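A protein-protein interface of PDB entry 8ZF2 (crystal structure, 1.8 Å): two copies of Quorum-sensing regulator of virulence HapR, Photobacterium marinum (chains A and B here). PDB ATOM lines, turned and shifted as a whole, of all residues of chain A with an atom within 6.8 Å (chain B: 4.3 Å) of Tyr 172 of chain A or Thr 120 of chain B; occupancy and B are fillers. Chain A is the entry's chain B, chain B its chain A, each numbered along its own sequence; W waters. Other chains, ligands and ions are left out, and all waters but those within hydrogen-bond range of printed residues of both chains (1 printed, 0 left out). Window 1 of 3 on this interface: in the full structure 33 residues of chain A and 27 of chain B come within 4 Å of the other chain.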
ATOM      1  N   LEU A 101      17.868 -15.920  -3.292  1.00  0.00           N
ATOM      2  CA  LEU A 101      18.446 -17.232  -3.564  1.00  0.00           C
ATOM      3  C   LEU A 101      18.318 -17.576  -5.042  1.00  0.00           C
ATOM      4  O   LEU A 101      19.281 -18.039  -5.670  1.00  0.00           O
ATOM      5  CB  LEU A 101      17.773 -18.294  -2.689  1.00  0.00           C
ATOM      6  CG  LEU A 101      18.217 -19.753  -2.852  1.00  0.00           C
ATOM      7  CD1 LEU A 101      18.147 -20.448  -1.504  1.00  0.00           C
ATOM      8  CD2 LEU A 101      17.352 -20.498  -3.861  1.00  0.00           C
ATOM      9  N   LYS A 113      26.766 -22.063  -4.483  1.00  0.00           N
ATOM     10  CA  LYS A 113      27.051 -23.438  -4.886  1.00  0.00           C
ATOM     11  C   LYS A 113      27.880 -24.146  -3.826  1.00  0.00           C
ATOM     12  O   LYS A 113      27.584 -25.285  -3.447  1.00  0.00           O
ATOM     13  CB  LYS A 113      27.780 -23.455  -6.233  1.00  0.00           C
ATOM     14  CG  LYS A 113      28.109 -24.861  -6.756  1.00  0.00           C
ATOM     15  CD  LYS A 113      29.540 -25.286  -6.423  1.00  0.00           C
ATOM     16  CE  LYS A 113      29.725 -26.792  -6.586  1.00  0.00           C
ATOM     17  NZ  LYS A 113      31.126 -27.221  -6.290  1.00  0.00           N
ATOM     18  N   PHE A 116      25.819 -24.907  -0.494  1.00  0.00           N
ATOM     19  CA  PHE A 116      24.977 -26.100  -0.494  1.00  0.00           C
ATOM     20  C   PHE A 116      25.801 -27.380  -0.588  1.00  0.00           C
ATOM     21  O   PHE A 116      25.417 -28.406  -0.013  1.00  0.00           O
ATOM     22  CB  PHE A 116      23.947 -26.011  -1.619  1.00  0.00           C
ATOM     23  CG  PHE A 116      22.653 -25.379  -1.187  1.00  0.00           C
ATOM     24  CD1 PHE A 116      21.819 -26.033  -0.298  1.00  0.00           C
ATOM     25  CD2 PHE A 116      22.286 -24.120  -1.643  1.00  0.00           C
ATOM     26  CE1 PHE A 116      20.631 -25.456   0.116  1.00  0.00           C
ATOM     27  CE2 PHE A 116      21.091 -23.534  -1.236  1.00  0.00           C
ATOM     28  CZ  PHE A 116      20.262 -24.203  -0.360  1.00  0.00           C
ATOM     29  N   GLU A 117      26.937 -27.341  -1.286  1.00  0.00           N
ATOM     30  CA  GLU A 117      27.835 -28.491  -1.290  1.00  0.00           C
ATOM     31  C   GLU A 117      28.387 -28.752   0.104  1.00  0.00           C
ATOM     32  O   GLU A 117      28.448 -29.902   0.563  1.00  0.00           O
ATOM     33  CB  GLU A 117      28.966 -28.250  -2.289  1.00  0.00           C
ATOM     34  CG  GLU A 117      30.117 -29.213  -2.167  1.00  0.00           C
ATOM     35  CD  GLU A 117      31.314 -28.785  -3.000  1.00  0.00           C
ATOM     36  OE1 GLU A 117      31.278 -27.680  -3.594  1.00  0.00           O
ATOM     37  OE2 GLU A 117      32.285 -29.559  -3.060  1.00  0.00           O
ATOM     38  N   TRP A 118      28.797 -27.686   0.788  1.00  0.00           N
ATOM     39  CA  TRP A 118      29.226 -27.773   2.179  1.00  0.00           C
ATOM     40  C   TRP A 118      28.166 -28.433   3.052  1.00  0.00           C
ATOM     41  O   TRP A 118      28.485 -29.285   3.891  1.00  0.00           O
ATOM     42  CB  TRP A 118      29.531 -26.359   2.672  1.00  0.00           C
ATOM     43  CG  TRP A 118      30.242 -26.207   3.973  1.00  0.00           C
ATOM     44  CD1 TRP A 118      30.901 -27.165   4.694  1.00  0.00           C
ATOM     45  CD2 TRP A 118      30.378 -24.985   4.702  1.00  0.00           C
ATOM     46  NE1 TRP A 118      31.432 -26.604   5.841  1.00  0.00           N
ATOM     47  CE2 TRP A 118      31.121 -25.267   5.864  1.00  0.00           C
ATOM     48  CE3 TRP A 118      29.927 -23.679   4.487  1.00  0.00           C
ATOM     49  CZ2 TRP A 118      31.432 -24.287   6.807  1.00  0.00           C
ATOM     50  CZ3 TRP A 118      30.243 -22.702   5.422  1.00  0.00           C
ATOM     51  CH2 TRP A 118      30.986 -23.016   6.568  1.00  0.00           C
ATOM     52  N   SER A 119      26.895 -28.066   2.854  1.00  0.00           N
ATOM     53  CA  SER A 119      25.834 -28.525   3.750  1.00  0.00           C
ATOM     54  C   SER A 119      25.682 -30.042   3.735  1.00  0.00           C
ATOM     55  O   SER A 119      25.225 -30.621   4.726  1.00  0.00           O
ATOM     56  CB  SER A 119      24.495 -27.873   3.384  1.00  0.00           C
ATOM     57  OG  SER A 119      23.907 -28.462   2.230  1.00  0.00           O
ATOM     58  N   THR A 120      26.041 -30.697   2.630  1.00  0.00           N
ATOM     59  CA  THR A 120      25.904 -32.142   2.497  1.00  0.00           C
ATOM     60  C   THR A 120      27.246 -32.865   2.527  1.00  0.00           C
ATOM     61  O   THR A 120      27.286 -34.080   2.310  1.00  0.00           O
ATOM     62  CB  THR A 120      25.161 -32.500   1.204  1.00  0.00           C
ATOM     63  OG1 THR A 120      25.885 -31.991   0.080  1.00  0.00           O
ATOM     64  CG2 THR A 120      23.761 -31.900   1.206  1.00  0.00           C
ATOM     65  N   SER A 121      28.341 -32.153   2.786  1.00  0.00           N
ATOM     66  CA  SER A 121      29.660 -32.779   2.888  1.00  0.00           C
ATOM     67  C   SER A 121      29.910 -33.183   4.341  1.00  0.00           C
ATOM     68  O   SER A 121      30.678 -32.565   5.076  1.00  0.00           O
ATOM     69  CB  SER A 121      30.736 -31.834   2.371  1.00  0.00           C
ATOM     70  OG  SER A 121      30.478 -31.470   1.028  1.00  0.00           O
ATOM     71  N   LEU A 167      11.802 -23.539   6.316  1.00  0.00           N
ATOM     72  CA  LEU A 167      12.212 -22.603   5.272  1.00  0.00           C
ATOM     73  C   LEU A 167      13.534 -23.027   4.649  1.00  0.00           C
ATOM     74  O   LEU A 167      13.760 -22.850   3.445  1.00  0.00           O
ATOM     75  CB  LEU A 167      12.323 -21.196   5.857  1.00  0.00           C
ATOM     76  CG  LEU A 167      12.896 -20.135   4.921  1.00  0.00           C
ATOM     77  CD1 LEU A 167      11.949 -19.924   3.750  1.00  0.00           C
ATOM     78  CD2 LEU A 167      13.137 -18.840   5.674  1.00  0.00           C
ATOM     79  N   TYR A 168      14.425 -23.587   5.460  1.00  0.00           N
ATOM     80  CA  TYR A 168      15.686 -24.094   4.940  1.00  0.00           C
ATOM     81  C   TYR A 168      15.459 -25.229   3.935  1.00  0.00           C
ATOM     82  O   TYR A 168      16.124 -25.289   2.893  1.00  0.00           O
ATOM     83  CB  TYR A 168      16.547 -24.513   6.130  1.00  0.00           C
ATOM     84  CG  TYR A 168      17.896 -25.077   5.814  1.00  0.00           C
ATOM     85  CD1 TYR A 168      18.586 -24.700   4.672  1.00  0.00           C
ATOM     86  CD2 TYR A 168      18.518 -25.940   6.704  1.00  0.00           C
ATOM     87  CE1 TYR A 168      19.841 -25.216   4.397  1.00  0.00           C
ATOM     88  CE2 TYR A 168      19.767 -26.445   6.449  1.00  0.00           C
ATOM     89  CZ  TYR A 168      20.427 -26.084   5.294  1.00  0.00           C
ATOM     90  OH  TYR A 168      21.680 -26.600   5.042  1.00  0.00           O
ATOM     91  N   GLY A 169      14.508 -26.121   4.210  1.00  0.00           N
ATOM     92  CA  GLY A 169      14.175 -27.147   3.230  1.00  0.00           C
ATOM     93  C   GLY A 169      13.592 -26.557   1.959  1.00  0.00           C
ATOM     94  O   GLY A 169      13.897 -27.009   0.850  1.00  0.00           O
ATOM     95  N   ILE A 170      12.752 -25.528   2.104  1.00  0.00           N
ATOM     96  CA  ILE A 170      12.230 -24.813   0.943  1.00  0.00           C
ATOM     97  C   ILE A 170      13.369 -24.223   0.118  1.00  0.00           C
ATOM     98  O   ILE A 170      13.346 -24.258  -1.120  1.00  0.00           O
ATOM     99  CB  ILE A 170      11.236 -23.729   1.405  1.00  0.00           C
ATOM    100  CG1 ILE A 170       9.936 -24.378   1.885  1.00  0.00           C
ATOM    101  CG2 ILE A 170      10.975 -22.717   0.288  1.00  0.00           C
ATOM    102  CD1 ILE A 170       8.995 -23.419   2.589  1.00  0.00           C
ATOM    103  N   CYS A 171      14.379 -23.665   0.787  1.00  0.00           N
ATOM    104  CA  CYS A 171      15.499 -23.077   0.061  1.00  0.00           C
ATOM    105  C   CYS A 171      16.277 -24.141  -0.704  1.00  0.00           C
ATOM    106  O   CYS A 171      16.725 -23.904  -1.831  1.00  0.00           O
ATOM    107  CB  CYS A 171      16.409 -22.330   1.033  1.00  0.00           C
ATOM    108  SG  CYS A 171      15.680 -20.789   1.613  1.00  0.00           S
ATOM    109  N   TYR A 172      16.435 -25.321  -0.104  1.00  0.00           N
ATOM    110  CA  TYR A 172      17.118 -26.417  -0.779  1.00  0.00           C
ATOM    111  C   TYR A 172      16.367 -26.846  -2.035  1.00  0.00           C
ATOM    112  O   TYR A 172      16.974 -27.020  -3.098  1.00  0.00           O
ATOM    113  CB  TYR A 172      17.282 -27.583   0.193  1.00  0.00           C
ATOM    114  CG  TYR A 172      17.735 -28.896  -0.405  1.00  0.00           C
ATOM    115  CD1 TYR A 172      19.058 -29.097  -0.785  1.00  0.00           C
ATOM    116  CD2 TYR A 172      16.839 -29.950  -0.557  1.00  0.00           C
ATOM    117  CE1 TYR A 172      19.474 -30.307  -1.307  1.00  0.00           C
ATOM    118  CE2 TYR A 172      17.247 -31.167  -1.078  1.00  0.00           C
ATOM    119  CZ  TYR A 172      18.563 -31.339  -1.454  1.00  0.00           C
ATOM    120  OH  TYR A 172      18.966 -32.548  -1.977  1.00  0.00           O
ATOM    121  N   VAL A 173      15.043 -27.002  -1.949  1.00  0.00           N
ATOM    122  CA  VAL A 173      14.334 -27.443  -3.151  1.00  0.00           C
ATOM    123  C   VAL A 173      14.272 -26.329  -4.188  1.00  0.00           C
ATOM    124  O   VAL A 173      14.321 -26.595  -5.394  1.00  0.00           O
ATOM    125  CB  VAL A 173      12.935 -27.990  -2.806  1.00  0.00           C
ATOM    126  CG1 VAL A 173      13.070 -29.259  -1.970  1.00  0.00           C
ATOM    127  CG2 VAL A 173      12.094 -26.953  -2.085  1.00  0.00           C
ATOM    128  N   LEU A 174      14.172 -25.069  -3.750  1.00  0.00           N
ATOM    129  CA  LEU A 174      14.233 -23.963  -4.699  1.00  0.00           C
ATOM    130  C   LEU A 174      15.593 -23.904  -5.376  1.00  0.00           C
ATOM    131  O   LEU A 174      15.689 -23.622  -6.575  1.00  0.00           O
ATOM    132  CB  LEU A 174      13.940 -22.640  -3.990  1.00  0.00           C
ATOM    133  CG  LEU A 174      12.478 -22.280  -3.731  1.00  0.00           C
ATOM    134  CD1 LEU A 174      12.394 -20.955  -2.986  1.00  0.00           C
ATOM    135  CD2 LEU A 174      11.663 -22.237  -5.031  1.00  0.00           C
ATOM    136  N   TYR A 175      16.658 -24.173  -4.621  1.00  0.00           N
ATOM    137  CA  TYR A 175      17.998 -24.190  -5.192  1.00  0.00           C
ATOM    138  C   TYR A 175      18.112 -25.237  -6.296  1.00  0.00           C
ATOM    139  O   TYR A 175      18.653 -24.965  -7.375  1.00  0.00           O
ATOM    140  CB  TYR A 175      19.017 -24.449  -4.083  1.00  0.00           C
ATOM    141  CG  TYR A 175      20.437 -24.604  -4.567  1.00  0.00           C
ATOM    142  CD1 TYR A 175      21.171 -23.505  -4.983  1.00  0.00           C
ATOM    143  CD2 TYR A 175      21.053 -25.847  -4.585  1.00  0.00           C
ATOM    144  CE1 TYR A 175      22.474 -23.638  -5.417  1.00  0.00           C
ATOM    145  CE2 TYR A 175      22.353 -25.990  -5.013  1.00  0.00           C
ATOM    146  CZ  TYR A 175      23.059 -24.879  -5.430  1.00  0.00           C
ATOM    147  OH  TYR A 175      24.354 -25.010  -5.863  1.00  0.00           O
ATOM    148  N   LEU A 176      17.593 -26.438  -6.046  1.00  0.00           N
ATOM    149  CA  LEU A 176      17.666 -27.496  -7.047  1.00  0.00           C
ATOM    150  C   LEU A 176      16.795 -27.170  -8.253  1.00  0.00           C
ATOM    151  O   LEU A 176      17.226 -27.319  -9.403  1.00  0.00           O
ATOM    152  CB  LEU A 176      17.242 -28.830  -6.428  1.00  0.00           C
ATOM    153  CG  LEU A 176      18.128 -29.347  -5.293  1.00  0.00           C
ATOM    154  CD1 LEU A 176      17.582 -30.657  -4.775  1.00  0.00           C
ATOM    155  CD2 LEU A 176      19.559 -29.527  -5.776  1.00  0.00           C
ATOM    156  N   GLN A 177      15.559 -26.730  -8.009  1.00  0.00           N
ATOM    157  CA  GLN A 177      14.657 -26.445  -9.118  1.00  0.00           C
ATOM    158  C   GLN A 177      15.148 -25.273  -9.958  1.00  0.00           C
ATOM    159  O   GLN A 177      14.954 -25.272 -11.179  1.00  0.00           O
ATOM    160  CB  GLN A 177      13.249 -26.182  -8.592  1.00  0.00           C
ATOM    161  CG  GLN A 177      12.588 -27.411  -7.994  1.00  0.00           C
ATOM    162  CD  GLN A 177      11.190 -27.124  -7.491  1.00  0.00           C
ATOM    163  OE1 GLN A 177      11.009 -26.428  -6.493  1.00  0.00           O
ATOM    164  NE2 GLN A 177      10.191 -27.642  -8.190  1.00  0.00           N
ATOM    165  N   PHE B 116      22.893 -37.535  -0.982  1.00  0.00           N
ATOM    166  CA  PHE B 116      22.708 -36.116  -0.704  1.00  0.00           C
ATOM    167  C   PHE B 116      23.877 -35.283  -1.219  1.00  0.00           C
ATOM    168  O   PHE B 116      23.681 -34.156  -1.683  1.00  0.00           O
ATOM    169  CB  PHE B 116      22.473 -35.898   0.786  1.00  0.00           C
ATOM    170  CG  PHE B 116      21.018 -35.891   1.154  1.00  0.00           C
ATOM    171  CD1 PHE B 116      20.199 -34.850   0.749  1.00  0.00           C
ATOM    172  CD2 PHE B 116      20.463 -36.927   1.883  1.00  0.00           C
ATOM    173  CE1 PHE B 116      18.852 -34.839   1.068  1.00  0.00           C
ATOM    174  CE2 PHE B 116      19.122 -36.921   2.208  1.00  0.00           C
ATOM    175  CZ  PHE B 116      18.314 -35.872   1.800  1.00  0.00           C
ATOM    176  N   GLU B 117      25.098 -35.817  -1.170  1.00  0.00           N
ATOM    177  CA  GLU B 117      26.215 -35.091  -1.763  1.00  0.00           C
ATOM    178  C   GLU B 117      26.054 -34.990  -3.280  1.00  0.00           C
ATOM    179  O   GLU B 117      26.348 -33.950  -3.880  1.00  0.00           O
ATOM    180  CB  GLU B 117      27.532 -35.773  -1.393  1.00  0.00           C
ATOM    181  CG  GLU B 117      28.679 -35.411  -2.302  1.00  0.00           C
ATOM    182  CD  GLU B 117      29.982 -36.073  -1.900  1.00  0.00           C
ATOM    183  OE1 GLU B 117      29.969 -36.937  -0.992  1.00  0.00           O
ATOM    184  OE2 GLU B 117      31.013 -35.734  -2.508  1.00  0.00           O
ATOM    185  N   TRP B 118      25.576 -36.067  -3.908  1.00  0.00           N
ATOM    186  CA  TRP B 118      25.250 -36.048  -5.330  1.00  0.00           C
ATOM    187  C   TRP B 118      24.256 -34.938  -5.657  1.00  0.00           C
ATOM    188  O   TRP B 118      24.399 -34.242  -6.672  1.00  0.00           O
ATOM    189  CB  TRP B 118      24.686 -37.417  -5.710  1.00  0.00           C
ATOM    190  CG  TRP B 118      24.528 -37.749  -7.161  1.00  0.00           C
ATOM    191  CD1 TRP B 118      25.050 -37.090  -8.239  1.00  0.00           C
ATOM    192  CD2 TRP B 118      23.788 -38.854  -7.683  1.00  0.00           C
ATOM    193  NE1 TRP B 118      24.671 -37.723  -9.405  1.00  0.00           N
ATOM    194  CE2 TRP B 118      23.892 -38.807  -9.087  1.00  0.00           C
ATOM    195  CE3 TRP B 118      23.029 -39.874  -7.096  1.00  0.00           C
ATOM    196  CZ2 TRP B 118      23.275 -39.745  -9.913  1.00  0.00           C
ATOM    197  CZ3 TRP B 118      22.418 -40.806  -7.919  1.00  0.00           C
ATOM    198  CH2 TRP B 118      22.546 -40.736  -9.312  1.00  0.00           C
ATOM    199  N   SER B 119      23.254 -34.742  -4.792  1.00  0.00           N
ATOM    200  CA  SER B 119      22.180 -33.797  -5.094  1.00  0.00           C
ATOM    201  C   SER B 119      22.685 -32.366  -5.221  1.00  0.00           C
ATOM    202  O   SER B 119      22.078 -31.561  -5.939  1.00  0.00           O
ATOM    203  CB  SER B 119      21.083 -33.868  -4.022  1.00  0.00           C
ATOM    204  OG  SER B 119      21.493 -33.288  -2.796  1.00  0.00           O
ATOM    205  N   THR B 120      23.778 -32.018  -4.540  1.00  0.00           N
ATOM    206  CA  THR B 120      24.279 -30.649  -4.570  1.00  0.00           C
ATOM    207  C   THR B 120      25.561 -30.508  -5.388  1.00  0.00           C
ATOM    208  O   THR B 120      26.253 -29.495  -5.270  1.00  0.00           O
ATOM    209  CB  THR B 120      24.489 -30.118  -3.148  1.00  0.00           C
ATOM    210  OG1 THR B 120      25.377 -30.979  -2.424  1.00  0.00           O
ATOM    211  CG2 THR B 120      23.153 -30.056  -2.418  1.00  0.00           C
ATOM    212  N   SER B 121      25.884 -31.496  -6.225  1.00  0.00           N
ATOM    213  CA  SER B 121      27.061 -31.426  -7.099  1.00  0.00           C
ATOM    214  C   SER B 121      26.699 -30.763  -8.429  1.00  0.00           C
ATOM    215  O   SER B 121      26.791 -31.357  -9.500  1.00  0.00           O
ATOM    216  CB  SER B 121      27.641 -32.817  -7.322  1.00  0.00           C
ATOM    217  OG  SER B 121      27.913 -33.456  -6.087  1.00  0.00           O
ATOM    218  N   ILE B 122      26.314 -29.486  -8.332  1.00  0.00           N
ATOM    219  CA  ILE B 122      25.655 -28.797  -9.441  1.00  0.00           C
ATOM    220  C   ILE B 122      26.569 -28.734 -10.659  1.00  0.00           C
ATOM    221  O   ILE B 122      26.152 -29.009 -11.791  1.00  0.00           O
ATOM    222  CB  ILE B 122      25.230 -27.379  -9.014  1.00  0.00           C
ATOM    223  CG1 ILE B 122      24.057 -27.394  -8.032  1.00  0.00           C
ATOM    224  CG2 ILE B 122      24.865 -26.542 -10.238  1.00  0.00           C
ATOM    225  CD1 ILE B 122      23.124 -28.512  -8.182  1.00  0.00           C
ATOM    226  N   TYR B 168      10.498 -33.612  -0.198  1.00  0.00           N
ATOM    227  CA  TYR B 168      11.929 -33.710  -0.450  1.00  0.00           C
ATOM    228  C   TYR B 168      12.700 -32.727   0.426  1.00  0.00           C
ATOM    229  O   TYR B 168      13.711 -33.086   1.044  1.00  0.00           O
ATOM    230  CB  TYR B 168      12.180 -33.462  -1.938  1.00  0.00           C
ATOM    231  CG  TYR B 168      13.613 -33.540  -2.396  1.00  0.00           C
ATOM    232  CD1 TYR B 168      13.988 -32.991  -3.612  1.00  0.00           C
ATOM    233  CD2 TYR B 168      14.581 -34.192  -1.642  1.00  0.00           C
ATOM    234  CE1 TYR B 168      15.285 -33.059  -4.053  1.00  0.00           C
ATOM    235  CE2 TYR B 168      15.886 -34.260  -2.077  1.00  0.00           C
ATOM    236  CZ  TYR B 168      16.234 -33.693  -3.284  1.00  0.00           C
ATOM    237  OH  TYR B 168      17.532 -33.752  -3.739  1.00  0.00           O
ATOM    238  N   TYR B 172      15.501 -33.368   3.427  1.00  0.00           N
ATOM    239  CA  TYR B 172      16.813 -32.730   3.512  1.00  0.00           C
ATOM    240  C   TYR B 172      17.071 -32.177   4.908  1.00  0.00           C
ATOM    241  O   TYR B 172      18.152 -32.379   5.474  1.00  0.00           O
ATOM    242  CB  TYR B 172      16.916 -31.627   2.462  1.00  0.00           C
ATOM    243  CG  TYR B 172      18.098 -30.687   2.583  1.00  0.00           C
ATOM    244  CD1 TYR B 172      19.387 -31.093   2.245  1.00  0.00           C
ATOM    245  CD2 TYR B 172      17.915 -29.377   3.000  1.00  0.00           C
ATOM    246  CE1 TYR B 172      20.462 -30.211   2.329  1.00  0.00           C
ATOM    247  CE2 TYR B 172      18.967 -28.499   3.086  1.00  0.00           C
ATOM    248  CZ  TYR B 172      20.239 -28.911   2.748  1.00  0.00           C
ATOM    249  OH  TYR B 172      21.276 -28.007   2.849  1.00  0.00           O
HETATM  250  O   HOH W   1      25.850 -26.964  -4.635  1.00  0.00           O
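OH of Tyr 172 of chain A lies within hydrogen-bond range of OG of Ser 119 of chain B (2.8 Å).
The side-chain hydroxyl of Thr 120 of chain B sits at hydrogen-bond distance from the side-chain hydroxyl of Thr 120 of chain A (2.7 Å).
The side-chain hydroxyl (OH) of Tyr 168 of chain B lies within hydrogen-bond range of the side-chain hydroxyl (OH) of Tyr 172 of chain A (2.6 Å).
OH of Tyr 172 of chain B lies within hydrogen-bond range of OG of Ser 119 of chain A (2.7 Å).
The side-chain hydroxyl of Tyr 168 of chain A sits at hydrogen-bond distance from the side-chain hydroxyl of Tyr 172 of chain B (2.6 Å).
The backbone carbonyl oxygen (O) of Phe 116 of chain B lies within hydrogen-bond range of the side-chain hydroxyl (OG) of Ser 119 of chain B, 2.6 Å away.
O of Glu 117 of chain B lies within hydrogen-bond range of OG1 of Thr 120 of chain B (3.4 Å).
The side-chain hydroxyl (OG) of Ser 121 of chain B sits at hydrogen-bond distance from the backbone carbonyl oxygen (O) of Glu 117 of chain B (2.8 Å).
The side-chain amino group (NZ) of Lys 113 of chain A is in salt-bridge range of the side-chain carboxylate (OE1) of Glu 117 of chain A (2.7 Å).
O of Phe 116 of chain A sits at hydrogen-bond distance from OG of Ser 119 of chain A (2.7 Å).
O of Glu 117 of chain A is in hydrogen-bond range of OG of Ser 121 of chain A (2.6 Å).
O of Phe 116 of chain A touches OG1 of Thr 120 of chain B (3.5 Å).
Tyr 172 of chain B touches Phe 116 of chain A (OH to CD1, 3.8 Å).
Phe 116 of chain B touches Thr 120 of chain A.
Thr 120 of chain A touches Glu 117 of chain B.
CE1 of Tyr 172 of chain B touches CG2 of Thr 120 of chain A, 3.9 Å away.
CE1 of Tyr 172 of chain A touches CG2 of Thr 120 of chain B, at 3.9 Å.
Tyr 172 of chain A touches Tyr 172 of chain B (CB to CD2, 3.4 Å).
Ile 122 of chain B touches Tyr 175 of chain A (CG1 to OH, 3.2 Å).
Leu 176 of chain A touches Ser 119 of chain B (CD2 to O, 3.2 Å).
CD1 of Leu 176 of chain A touches OH of Tyr 168 of chain B, 3.3 Å away.
Of the printed residues of chain B, Ser 119 of chain A touches Tyr 172.
Leu 167 of chain A touches none of the printed residues of chain B.
Tyr 172 of chain A touches just these residues of chain B: Phe 116 (3.8 Å), Ser 119 (2.8 Å), Thr 120 (3.9 Å), Tyr 168 (2.6 Å) and Tyr 172 (3.4 Å).
Of the printed residues of chain B, Leu 176 of chain A touches Ser 119 and Tyr 168.
Printed residues of chain A within 4 Å of Glu 117 of chain B: Thr 120 (3.6 Å).
Of the printed residues of chain A, Thr 120 of chain B touches Phe 116, Glu 117, Thr 120 and Tyr 172.
Of the printed residues of chain A, Tyr 168 of chain B touches Tyr 172 (2.6 Å) and Leu 176 (3.3 Å).
Of the printed residues of chain A, Tyr 172 of chain B touches Phe 116 (3.8 Å), Ser 119 (2.7 Å), Thr 120 (3.9 Å), Tyr 168 (2.6 Å) and Tyr 172 (3.4 Å).
The nearest printed residue of chain B that does not touch Tyr 172 of chain A is Trp 118 of chain B (6.9 Å).
The nearest residue of chain A that does not touch Thr 120 of chain B is Lys 113 of chain A (4.6 Å).
The nearest printed residue of chain A that does not touch Tyr 172 of chain B is Gly 169 of chain A (4.4 Å).
Hydrophobic or aromatic side chains of chain A that line the printed part of chain B: Phe 116, Tyr 168, Tyr 172, Tyr 175 and Leu 176.
Among the printed residues, 17 pairs touch across the chains.
Thr 120 of chain A touches its own counterpart, Thr 120 of chain B.
Thr 120 of chain A touches Tyr 172 of chain B, and with the chains exchanged Tyr 172 of chain A touches Thr 120 of chain B.
Tyr 168 of chain A touches Tyr 172 of chain B, and with the chains exchanged Tyr 172 of chain A touches Tyr 168 of chain B.
Tyr 172 of chain A touches its own counterpart, Tyr 172 of chain B.
8 positions are printed for both chains.
Of the 17 pairs that touch across the chains among the printed residues, 14 have their exchanged pair printed and touching as well.
Water W1 lies within hydrogen-bond range of the backbone carbonyl oxygen of Thr 120 of chain B (2.6 Å), the backbone carbonyl oxygen of Lys 113 of chain A (2.7 Å) and the side-chain hydroxyl of Tyr 175 of chain A (2.8 Å).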
